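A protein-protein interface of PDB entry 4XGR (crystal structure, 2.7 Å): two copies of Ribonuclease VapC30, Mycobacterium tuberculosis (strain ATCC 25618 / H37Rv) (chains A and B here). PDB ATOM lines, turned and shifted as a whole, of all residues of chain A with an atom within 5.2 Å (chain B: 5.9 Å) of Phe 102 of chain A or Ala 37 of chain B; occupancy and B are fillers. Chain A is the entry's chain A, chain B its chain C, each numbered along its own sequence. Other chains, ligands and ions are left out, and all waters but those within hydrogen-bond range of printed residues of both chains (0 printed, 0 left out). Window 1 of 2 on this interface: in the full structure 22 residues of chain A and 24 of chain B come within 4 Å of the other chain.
Among the printed residues, no Asp or Glu carboxylate lies within 4 Å of a Lys or Arg side-chain nitrogen of the other chain.
Among the printed residues, pairs that only touch across the chains: Ala 37 of chain A with Phe 102 of chain B, Phe 102 of chain A with Tyr 98 of chain B, Phe 102 of chain A with Ala 37 of chain B, Tyr 98 of chain A with Glu 41 of chain B, Phe 102 of chain A with Leu 40 of chain B, Tyr 98 of chain A with Phe 102 of chain B, Tyr 98 of chain A with Gly 99 of chain B and Tyr 98 of chain A with Tyr 98 of chain B.
The side-chain hydroxyl (OH) of Tyr 98 of chain A sits at hydrogen-bond distance from the backbone carbonyl oxygen (O) of Ala 37 of chain B, 2.8 Å away.
The side-chain hydroxyl (OH) of Tyr 98 of chain B lies close to the backbone carbonyl oxygen (O) of Ala 37 of chain A, at 2.3 Å.
N of Val 72 of chain A sits at hydrogen-bond distance from O of Val 72 of chain B (3.4 Å).
The backbone carbonyl oxygen (O) of Val 72 of chain A sits at hydrogen-bond distance from the side-chain hydroxyl (OG1) of Thr 36 of chain B (2.6 Å).
OE2 of Glu 41 of chain B is in hydrogen-bond range of OG1 of Thr 6 of chain B (3.3 Å).
N of Thr 36 of chain B lies within hydrogen-bond range of O of Val 70 of chain B (3.0 Å).
SG of Cys 101 of chain A lies close to O of Tyr 98 of chain A (3.7 Å).
Printed residues of chain B within 4 Å of Ala 37 of chain A: Tyr 98 (2.3 Å) and Phe 102 (3.4 Å).
Of chain B, only Ala 37, Leu 40 and Tyr 98 come within 4 Å of Phe 102 of chain A.
Of chain A, only Tyr 98 (2.8 Å) and Phe 102 (3.6 Å) come within 4 Å of Ala 37 of chain B.
Of the printed residues of chain A, Leu 40 of chain B touches Phe 102 (3.8 Å).
Of the printed residues of chain A, Val 72 of chain B touches Val 72 (3.4 Å).
Of the printed residues of chain A, Phe 102 of chain B touches Ala 37 (3.4 Å) and Tyr 98 (3.9 Å).
Ala 37 of chain A touches Tyr 98 of chain B, and with the chains exchanged Tyr 98 of chain A touches Ala 37 of chain B.
Val 72 of chain A touches its own counterpart, Val 72 of chain B.
Tyr 98 of chain B touches its own counterpart, Tyr 98 of chain A.
Tyr 98 of chain A touches Gly 99 of chain B, but with the chains exchanged Gly 99 of chain A does not touch Tyr 98 of chain B (4.2 Å).
7 positions are printed for both chains.
Of the 12 pairs that touch across the chains among the printed residues, 8 have their exchanged pair printed and touching as well.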
ATOM      1  N   SER A  35     -29.660 -13.457   1.603  1.00  0.00           N
ATOM      2  CA  SER A  35     -28.781 -14.609   1.441  1.00  0.00           C
ATOM      3  C   SER A  35     -29.210 -15.680   2.407  1.00  0.00           C
ATOM      4  O   SER A  35     -29.657 -15.379   3.529  1.00  0.00           O
ATOM      5  CB  SER A  35     -27.284 -14.285   1.656  1.00  0.00           C
ATOM      6  OG  SER A  35     -26.525 -14.716   0.511  1.00  0.00           O
ATOM      7  N   ALA A  37     -27.448 -17.602   4.039  1.00  0.00           N
ATOM      8  CA  ALA A  37     -26.548 -17.590   5.186  1.00  0.00           C
ATOM      9  C   ALA A  37     -26.909 -16.485   6.193  1.00  0.00           C
ATOM     10  O   ALA A  37     -26.619 -16.595   7.403  1.00  0.00           O
ATOM     11  CB  ALA A  37     -25.118 -17.399   4.684  1.00  0.00           C
ATOM     12  N   SER A  38     -27.483 -15.398   5.690  1.00  0.00           N
ATOM     13  CA  SER A  38     -28.078 -14.385   6.552  1.00  0.00           C
ATOM     14  C   SER A  38     -29.455 -14.831   7.092  1.00  0.00           C
ATOM     15  O   SER A  38     -29.766 -14.558   8.250  1.00  0.00           O
ATOM     16  CB  SER A  38     -28.134 -13.051   5.825  1.00  0.00           C
ATOM     17  OG  SER A  38     -26.821 -12.514   5.671  1.00  0.00           O
ATOM     18  N   VAL A  72     -25.819 -18.610  -2.065  1.00  0.00           N
ATOM     19  CA  VAL A  72     -24.541 -17.926  -1.877  1.00  0.00           C
ATOM     20  C   VAL A  72     -23.558 -18.445  -2.934  1.00  0.00           C
ATOM     21  O   VAL A  72     -22.709 -19.293  -2.646  1.00  0.00           O
ATOM     22  CB  VAL A  72     -23.974 -18.184  -0.453  1.00  0.00           C
ATOM     23  CG1 VAL A  72     -22.694 -17.393  -0.197  1.00  0.00           C
ATOM     24  CG2 VAL A  72     -24.988 -17.813   0.600  1.00  0.00           C
ATOM     25  N   GLN A  76     -20.286 -14.112  -5.211  1.00  0.00           N
ATOM     26  CA  GLN A  76     -20.590 -13.297  -4.030  1.00  0.00           C
ATOM     27  C   GLN A  76     -19.485 -13.480  -2.990  1.00  0.00           C
ATOM     28  O   GLN A  76     -18.911 -12.503  -2.479  1.00  0.00           O
ATOM     29  CB  GLN A  76     -21.959 -13.664  -3.406  1.00  0.00           C
ATOM     30  CG  GLN A  76     -23.183 -13.723  -4.333  1.00  0.00           C
ATOM     31  CD  GLN A  76     -24.419 -14.259  -3.619  1.00  0.00           C
ATOM     32  OE1 GLN A  76     -24.579 -14.044  -2.420  1.00  0.00           O
ATOM     33  NE2 GLN A  76     -25.303 -14.943  -4.349  1.00  0.00           N
ATOM     34  N   TYR A  98     -17.420 -12.120   9.612  1.00  0.00           N
ATOM     35  CA  TYR A  98     -17.661 -13.230   8.653  1.00  0.00           C
ATOM     36  C   TYR A  98     -19.108 -13.306   8.200  1.00  0.00           C
ATOM     37  O   TYR A  98     -19.352 -13.529   7.028  1.00  0.00           O
ATOM     38  CB  TYR A  98     -17.270 -14.577   9.271  1.00  0.00           C
ATOM     39  CG  TYR A  98     -17.700 -15.804   8.485  1.00  0.00           C
ATOM     40  CD1 TYR A  98     -17.312 -15.977   7.162  1.00  0.00           C
ATOM     41  CD2 TYR A  98     -18.475 -16.815   9.075  1.00  0.00           C
ATOM     42  CE1 TYR A  98     -17.687 -17.102   6.435  1.00  0.00           C
ATOM     43  CE2 TYR A  98     -18.850 -17.944   8.348  1.00  0.00           C
ATOM     44  CZ  TYR A  98     -18.440 -18.082   7.031  1.00  0.00           C
ATOM     45  OH  TYR A  98     -18.799 -19.177   6.284  1.00  0.00           O
ATOM     46  N   GLY A  99     -20.045 -13.131   9.145  1.00  0.00           N
ATOM     47  CA  GLY A  99     -21.490 -13.223   8.890  1.00  0.00           C
ATOM     48  C   GLY A  99     -22.020 -12.130   8.000  1.00  0.00           C
ATOM     49  O   GLY A  99     -22.757 -12.384   7.051  1.00  0.00           O
ATOM     50  N   ASP A 100     -21.621 -10.901   8.277  1.00  0.00           N
ATOM     51  CA  ASP A 100     -21.927  -9.755   7.396  1.00  0.00           C
ATOM     52  C   ASP A 100     -21.490  -9.968   5.947  1.00  0.00           C
ATOM     53  O   ASP A 100     -22.116  -9.426   5.048  1.00  0.00           O
ATOM     54  CB  ASP A 100     -21.251  -8.480   7.912  1.00  0.00           C
ATOM     55  CG  ASP A 100     -21.638  -8.135   9.342  1.00  0.00           C
ATOM     56  OD1 ASP A 100     -22.664  -8.630   9.856  1.00  0.00           O
ATOM     57  OD2 ASP A 100     -20.880  -7.375   9.964  1.00  0.00           O
ATOM     58  N   CYS A 101     -20.435 -10.747   5.718  1.00  0.00           N
ATOM     59  CA  CYS A 101     -19.966 -11.021   4.338  1.00  0.00           C
ATOM     60  C   CYS A 101     -21.005 -11.573   3.363  1.00  0.00           C
ATOM     61  O   CYS A 101     -20.882 -11.399   2.153  1.00  0.00           O
ATOM     62  CB  CYS A 101     -18.759 -11.967   4.346  1.00  0.00           C
ATOM     63  SG  CYS A 101     -17.255 -11.228   5.037  1.00  0.00           S
ATOM     64  N   PHE A 102     -22.024 -12.225   3.875  1.00  0.00           N
ATOM     65  CA  PHE A 102     -23.041 -12.877   3.035  1.00  0.00           C
ATOM     66  C   PHE A 102     -24.061 -11.879   2.486  1.00  0.00           C
ATOM     67  O   PHE A 102     -24.302 -11.821   1.255  1.00  0.00           O
ATOM     68  CB  PHE A 102     -23.698 -13.977   3.846  1.00  0.00           C
ATOM     69  CG  PHE A 102     -22.713 -14.994   4.324  1.00  0.00           C
ATOM     70  CD1 PHE A 102     -22.093 -15.827   3.410  1.00  0.00           C
ATOM     71  CD2 PHE A 102     -22.340 -15.072   5.666  1.00  0.00           C
ATOM     72  CE1 PHE A 102     -21.160 -16.746   3.822  1.00  0.00           C
ATOM     73  CE2 PHE A 102     -21.406 -16.001   6.083  1.00  0.00           C
ATOM     74  CZ  PHE A 102     -20.827 -16.844   5.149  1.00  0.00           C
ATOM     75  N   SER A 103     -24.620 -11.068   3.385  1.00  0.00           N
ATOM     76  CA  SER A 103     -25.457  -9.942   2.965  1.00  0.00           C
ATOM     77  C   SER A 103     -24.637  -8.948   2.145  1.00  0.00           C
ATOM     78  O   SER A 103     -25.117  -8.412   1.141  1.00  0.00           O
ATOM     79  CB  SER A 103     -26.143  -9.277   4.160  1.00  0.00           C
ATOM     80  OG  SER A 103     -27.325 -10.011   4.501  1.00  0.00           O
ATOM     81  N   TYR A 104     -23.387  -8.750   2.549  1.00  0.00           N
ATOM     82  CA  TYR A 104     -22.473  -7.939   1.780  1.00  0.00           C
ATOM     83  C   TYR A 104     -22.315  -8.465   0.361  1.00  0.00           C
ATOM     84  O   TYR A 104     -22.313  -7.667  -0.573  1.00  0.00           O
ATOM     85  CB  TYR A 104     -21.082  -7.868   2.421  1.00  0.00           C
ATOM     86  CG  TYR A 104     -20.185  -6.968   1.606  1.00  0.00           C
ATOM     87  CD1 TYR A 104     -20.152  -5.582   1.829  1.00  0.00           C
ATOM     88  CD2 TYR A 104     -19.435  -7.486   0.552  1.00  0.00           C
ATOM     89  CE1 TYR A 104     -19.375  -4.760   1.040  1.00  0.00           C
ATOM     90  CE2 TYR A 104     -18.655  -6.667  -0.244  1.00  0.00           C
ATOM     91  CZ  TYR A 104     -18.622  -5.307   0.006  1.00  0.00           C
ATOM     92  OH  TYR A 104     -17.829  -4.505  -0.776  1.00  0.00           O
ATOM     93  N   GLY A 105     -22.130  -9.782   0.204  1.00  0.00           N
ATOM     94  CA  GLY A 105     -21.868 -10.367  -1.110  1.00  0.00           C
ATOM     95  C   GLY A 105     -23.045 -10.222  -2.062  1.00  0.00           C
ATOM     96  O   GLY A 105     -22.874  -9.833  -3.229  1.00  0.00           O
ATOM     97  N   LEU A 106     -24.237 -10.545  -1.555  1.00  0.00           N
ATOM     98  CA  LEU A 106     -25.502 -10.434  -2.296  1.00  0.00           C
ATOM     99  C   LEU A 106     -25.778  -9.001  -2.756  1.00  0.00           C
ATOM    100  O   LEU A 106     -26.135  -8.791  -3.927  1.00  0.00           O
ATOM    101  CB  LEU A 106     -26.661 -10.918  -1.420  1.00  0.00           C
ATOM    102  CG  LEU A 106     -28.092 -10.863  -1.949  1.00  0.00           C
ATOM    103  CD1 LEU A 106     -28.189 -11.527  -3.319  1.00  0.00           C
ATOM    104  CD2 LEU A 106     -29.040 -11.526  -0.954  1.00  0.00           C
ATOM    105  N   ALA A 107     -25.600  -8.016  -1.864  1.00  0.00           N
ATOM    106  CA  ALA A 107     -25.790  -6.603  -2.263  1.00  0.00           C
ATOM    107  C   ALA A 107     -24.903  -6.196  -3.458  1.00  0.00           C
ATOM    108  O   ALA A 107     -25.407  -5.630  -4.435  1.00  0.00           O
ATOM    109  CB  ALA A 107     -25.559  -5.669  -1.097  1.00  0.00           C
ATOM    110  N   THR B   6     -13.423 -25.925   6.126  1.00  0.00           N
ATOM    111  CA  THR B   6     -12.371 -24.998   6.483  1.00  0.00           C
ATOM    112  C   THR B   6     -11.290 -25.543   7.424  1.00  0.00           C
ATOM    113  O   THR B   6     -10.161 -25.062   7.372  1.00  0.00           O
ATOM    114  CB  THR B   6     -13.001 -23.757   7.145  1.00  0.00           C
ATOM    115  OG1 THR B   6     -14.007 -23.244   6.272  1.00  0.00           O
ATOM    116  CG2 THR B   6     -11.961 -22.663   7.426  1.00  0.00           C
ATOM    117  N   SER B  35     -18.228 -25.956   0.102  1.00  0.00           N
ATOM    118  CA  SER B  35     -19.286 -24.959   0.229  1.00  0.00           C
ATOM    119  C   SER B  35     -18.704 -23.581   0.040  1.00  0.00           C
ATOM    120  O   SER B  35     -17.795 -23.177   0.777  1.00  0.00           O
ATOM    121  CB  SER B  35     -19.952 -25.034   1.615  1.00  0.00           C
ATOM    122  OG  SER B  35     -21.013 -24.094   1.724  1.00  0.00           O
ATOM    123  N   THR B  36     -19.267 -22.843  -0.909  1.00  0.00           N
ATOM    124  CA  THR B  36     -18.844 -21.464  -1.208  1.00  0.00           C
ATOM    125  C   THR B  36     -18.554 -20.600   0.025  1.00  0.00           C
ATOM    126  O   THR B  36     -17.820 -19.621  -0.053  1.00  0.00           O
ATOM    127  CB  THR B  36     -19.952 -20.729  -1.975  1.00  0.00           C
ATOM    128  OG1 THR B  36     -21.188 -20.903  -1.273  1.00  0.00           O
ATOM    129  CG2 THR B  36     -20.085 -21.238  -3.406  1.00  0.00           C
ATOM    130  N   ALA B  37     -19.201 -20.938   1.136  1.00  0.00           N
ATOM    131  CA  ALA B  37     -19.086 -20.209   2.385  1.00  0.00           C
ATOM    132  C   ALA B  37     -18.012 -20.797   3.302  1.00  0.00           C
ATOM    133  O   ALA B  37     -17.396 -20.067   4.074  1.00  0.00           O
ATOM    134  CB  ALA B  37     -20.449 -20.199   3.079  1.00  0.00           C
ATOM    135  N   SER B  38     -17.817 -22.112   3.252  1.00  0.00           N
ATOM    136  CA  SER B  38     -16.628 -22.732   3.863  1.00  0.00           C
ATOM    137  C   SER B  38     -15.345 -22.221   3.152  1.00  0.00           C
ATOM    138  O   SER B  38     -14.419 -21.751   3.802  1.00  0.00           O
ATOM    139  CB  SER B  38     -16.726 -24.252   3.799  1.00  0.00           C
ATOM    140  OG  SER B  38     -17.918 -24.716   4.425  1.00  0.00           O
ATOM    141  N   TYR B  39     -15.333 -22.281   1.821  1.00  0.00           N
ATOM    142  CA  TYR B  39     -14.298 -21.618   1.005  1.00  0.00           C
ATOM    143  C   TYR B  39     -14.035 -20.149   1.395  1.00  0.00           C
ATOM    144  O   TYR B  39     -12.878 -19.720   1.501  1.00  0.00           O
ATOM    145  CB  TYR B  39     -14.632 -21.741  -0.501  1.00  0.00           C
ATOM    146  CG  TYR B  39     -14.170 -20.581  -1.350  1.00  0.00           C
ATOM    147  CD1 TYR B  39     -12.811 -20.330  -1.552  1.00  0.00           C
ATOM    148  CD2 TYR B  39     -15.099 -19.725  -1.955  1.00  0.00           C
ATOM    149  CE1 TYR B  39     -12.395 -19.238  -2.319  1.00  0.00           C
ATOM    150  CE2 TYR B  39     -14.699 -18.655  -2.736  1.00  0.00           C
ATOM    151  CZ  TYR B  39     -13.353 -18.409  -2.912  1.00  0.00           C
ATOM    152  OH  TYR B  39     -12.964 -17.353  -3.673  1.00  0.00           O
ATOM    153  N   LEU B  40     -15.103 -19.388   1.604  1.00  0.00           N
ATOM    154  CA  LEU B  40     -14.996 -17.993   2.044  1.00  0.00           C
ATOM    155  C   LEU B  40     -14.380 -17.863   3.428  1.00  0.00           C
ATOM    156  O   LEU B  40     -13.455 -17.095   3.618  1.00  0.00           O
ATOM    157  CB  LEU B  40     -16.371 -17.329   2.034  1.00  0.00           C
ATOM    158  CG  LEU B  40     -16.458 -15.905   2.597  1.00  0.00           C
ATOM    159  CD1 LEU B  40     -15.496 -14.954   1.881  1.00  0.00           C
ATOM    160  CD2 LEU B  40     -17.909 -15.420   2.498  1.00  0.00           C
ATOM    161  N   GLU B  41     -14.911 -18.593   4.401  1.00  0.00           N
ATOM    162  CA  GLU B  41     -14.290 -18.675   5.745  1.00  0.00           C
ATOM    163  C   GLU B  41     -12.788 -19.033   5.650  1.00  0.00           C
ATOM    164  O   GLU B  41     -11.948 -18.493   6.367  1.00  0.00           O
ATOM    165  CB  GLU B  41     -15.017 -19.731   6.591  1.00  0.00           C
ATOM    166  CG  GLU B  41     -14.641 -19.762   8.069  1.00  0.00           C
ATOM    167  CD  GLU B  41     -15.368 -20.838   8.856  1.00  0.00           C
ATOM    168  OE1 GLU B  41     -15.212 -20.810  10.088  1.00  0.00           O
ATOM    169  OE2 GLU B  41     -16.099 -21.688   8.271  1.00  0.00           O
ATOM    170  N   THR B  42     -12.483 -19.961   4.752  1.00  0.00           N
ATOM    171  CA  THR B  42     -11.126 -20.382   4.477  1.00  0.00           C
ATOM    172  C   THR B  42     -10.308 -19.262   3.833  1.00  0.00           C
ATOM    173  O   THR B  42      -9.159 -19.043   4.196  1.00  0.00           O
ATOM    174  CB  THR B  42     -11.145 -21.602   3.551  1.00  0.00           C
ATOM    175  OG1 THR B  42     -11.974 -22.617   4.132  1.00  0.00           O
ATOM    176  CG2 THR B  42      -9.738 -22.142   3.322  1.00  0.00           C
ATOM    177  N   VAL B  70     -19.777 -25.506  -4.255  1.00  0.00           N
ATOM    178  CA  VAL B  70     -21.233 -25.659  -4.299  1.00  0.00           C
ATOM    179  C   VAL B  70     -21.936 -24.516  -3.579  1.00  0.00           C
ATOM    180  O   VAL B  70     -21.507 -24.058  -2.510  1.00  0.00           O
ATOM    181  CB  VAL B  70     -21.694 -26.996  -3.727  1.00  0.00           C
ATOM    182  CG1 VAL B  70     -23.200 -27.175  -3.970  1.00  0.00           C
ATOM    183  CG2 VAL B  70     -20.884 -28.146  -4.349  1.00  0.00           C
ATOM    184  N   VAL B  72     -24.692 -22.452  -1.468  1.00  0.00           N
ATOM    185  CA  VAL B  72     -25.492 -22.657  -0.285  1.00  0.00           C
ATOM    186  C   VAL B  72     -26.917 -22.467  -0.753  1.00  0.00           C
ATOM    187  O   VAL B  72     -27.409 -21.348  -0.814  1.00  0.00           O
ATOM    188  CB  VAL B  72     -25.160 -21.640   0.823  1.00  0.00           C
ATOM    189  CG1 VAL B  72     -25.999 -21.938   2.059  1.00  0.00           C
ATOM    190  CG2 VAL B  72     -23.670 -21.669   1.156  1.00  0.00           C
ATOM    191  N   TYR B  98     -21.493 -21.595  13.563  1.00  0.00           N
ATOM    192  CA  TYR B  98     -22.147 -20.998  12.419  1.00  0.00           C
ATOM    193  C   TYR B  98     -21.357 -21.350  11.175  1.00  0.00           C
ATOM    194  O   TYR B  98     -21.938 -21.822  10.205  1.00  0.00           O
ATOM    195  CB  TYR B  98     -22.274 -19.475  12.579  1.00  0.00           C
ATOM    196  CG  TYR B  98     -22.847 -18.789  11.354  1.00  0.00           C
ATOM    197  CD1 TYR B  98     -24.113 -19.086  10.901  1.00  0.00           C
ATOM    198  CD2 TYR B  98     -22.107 -17.858  10.645  1.00  0.00           C
ATOM    199  CE1 TYR B  98     -24.634 -18.469   9.771  1.00  0.00           C
ATOM    200  CE2 TYR B  98     -22.615 -17.238   9.520  1.00  0.00           C
ATOM    201  CZ  TYR B  98     -23.875 -17.549   9.081  1.00  0.00           C
ATOM    202  OH  TYR B  98     -24.377 -16.927   7.966  1.00  0.00           O
ATOM    203  N   GLY B  99     -20.039 -21.140  11.205  1.00  0.00           N
ATOM    204  CA  GLY B  99     -19.166 -21.484  10.068  1.00  0.00           C
ATOM    205  C   GLY B  99     -19.261 -22.950   9.672  1.00  0.00           C
ATOM    206  O   GLY B  99     -19.292 -23.292   8.490  1.00  0.00           O
ATOM    207  N   PHE B 102     -22.367 -24.683   7.226  1.00  0.00           N
ATOM    208  CA  PHE B 102     -22.381 -24.820   5.745  1.00  0.00           C
ATOM    209  C   PHE B 102     -21.735 -26.124   5.276  1.00  0.00           C
ATOM    210  O   PHE B 102     -22.103 -26.667   4.225  1.00  0.00           O
ATOM    211  CB  PHE B 102     -21.737 -23.602   5.067  1.00  0.00           C
ATOM    212  CG  PHE B 102     -22.367 -22.323   5.472  1.00  0.00           C
ATOM    213  CD1 PHE B 102     -23.508 -21.871   4.832  1.00  0.00           C
ATOM    214  CD2 PHE B 102     -21.858 -21.596   6.545  1.00  0.00           C
ATOM    215  CE1 PHE B 102     -24.119 -20.702   5.244  1.00  0.00           C
ATOM    216  CE2 PHE B 102     -22.461 -20.431   6.954  1.00  0.00           C
ATOM    217  CZ  PHE B 102     -23.594 -19.987   6.306  1.00  0.00           C
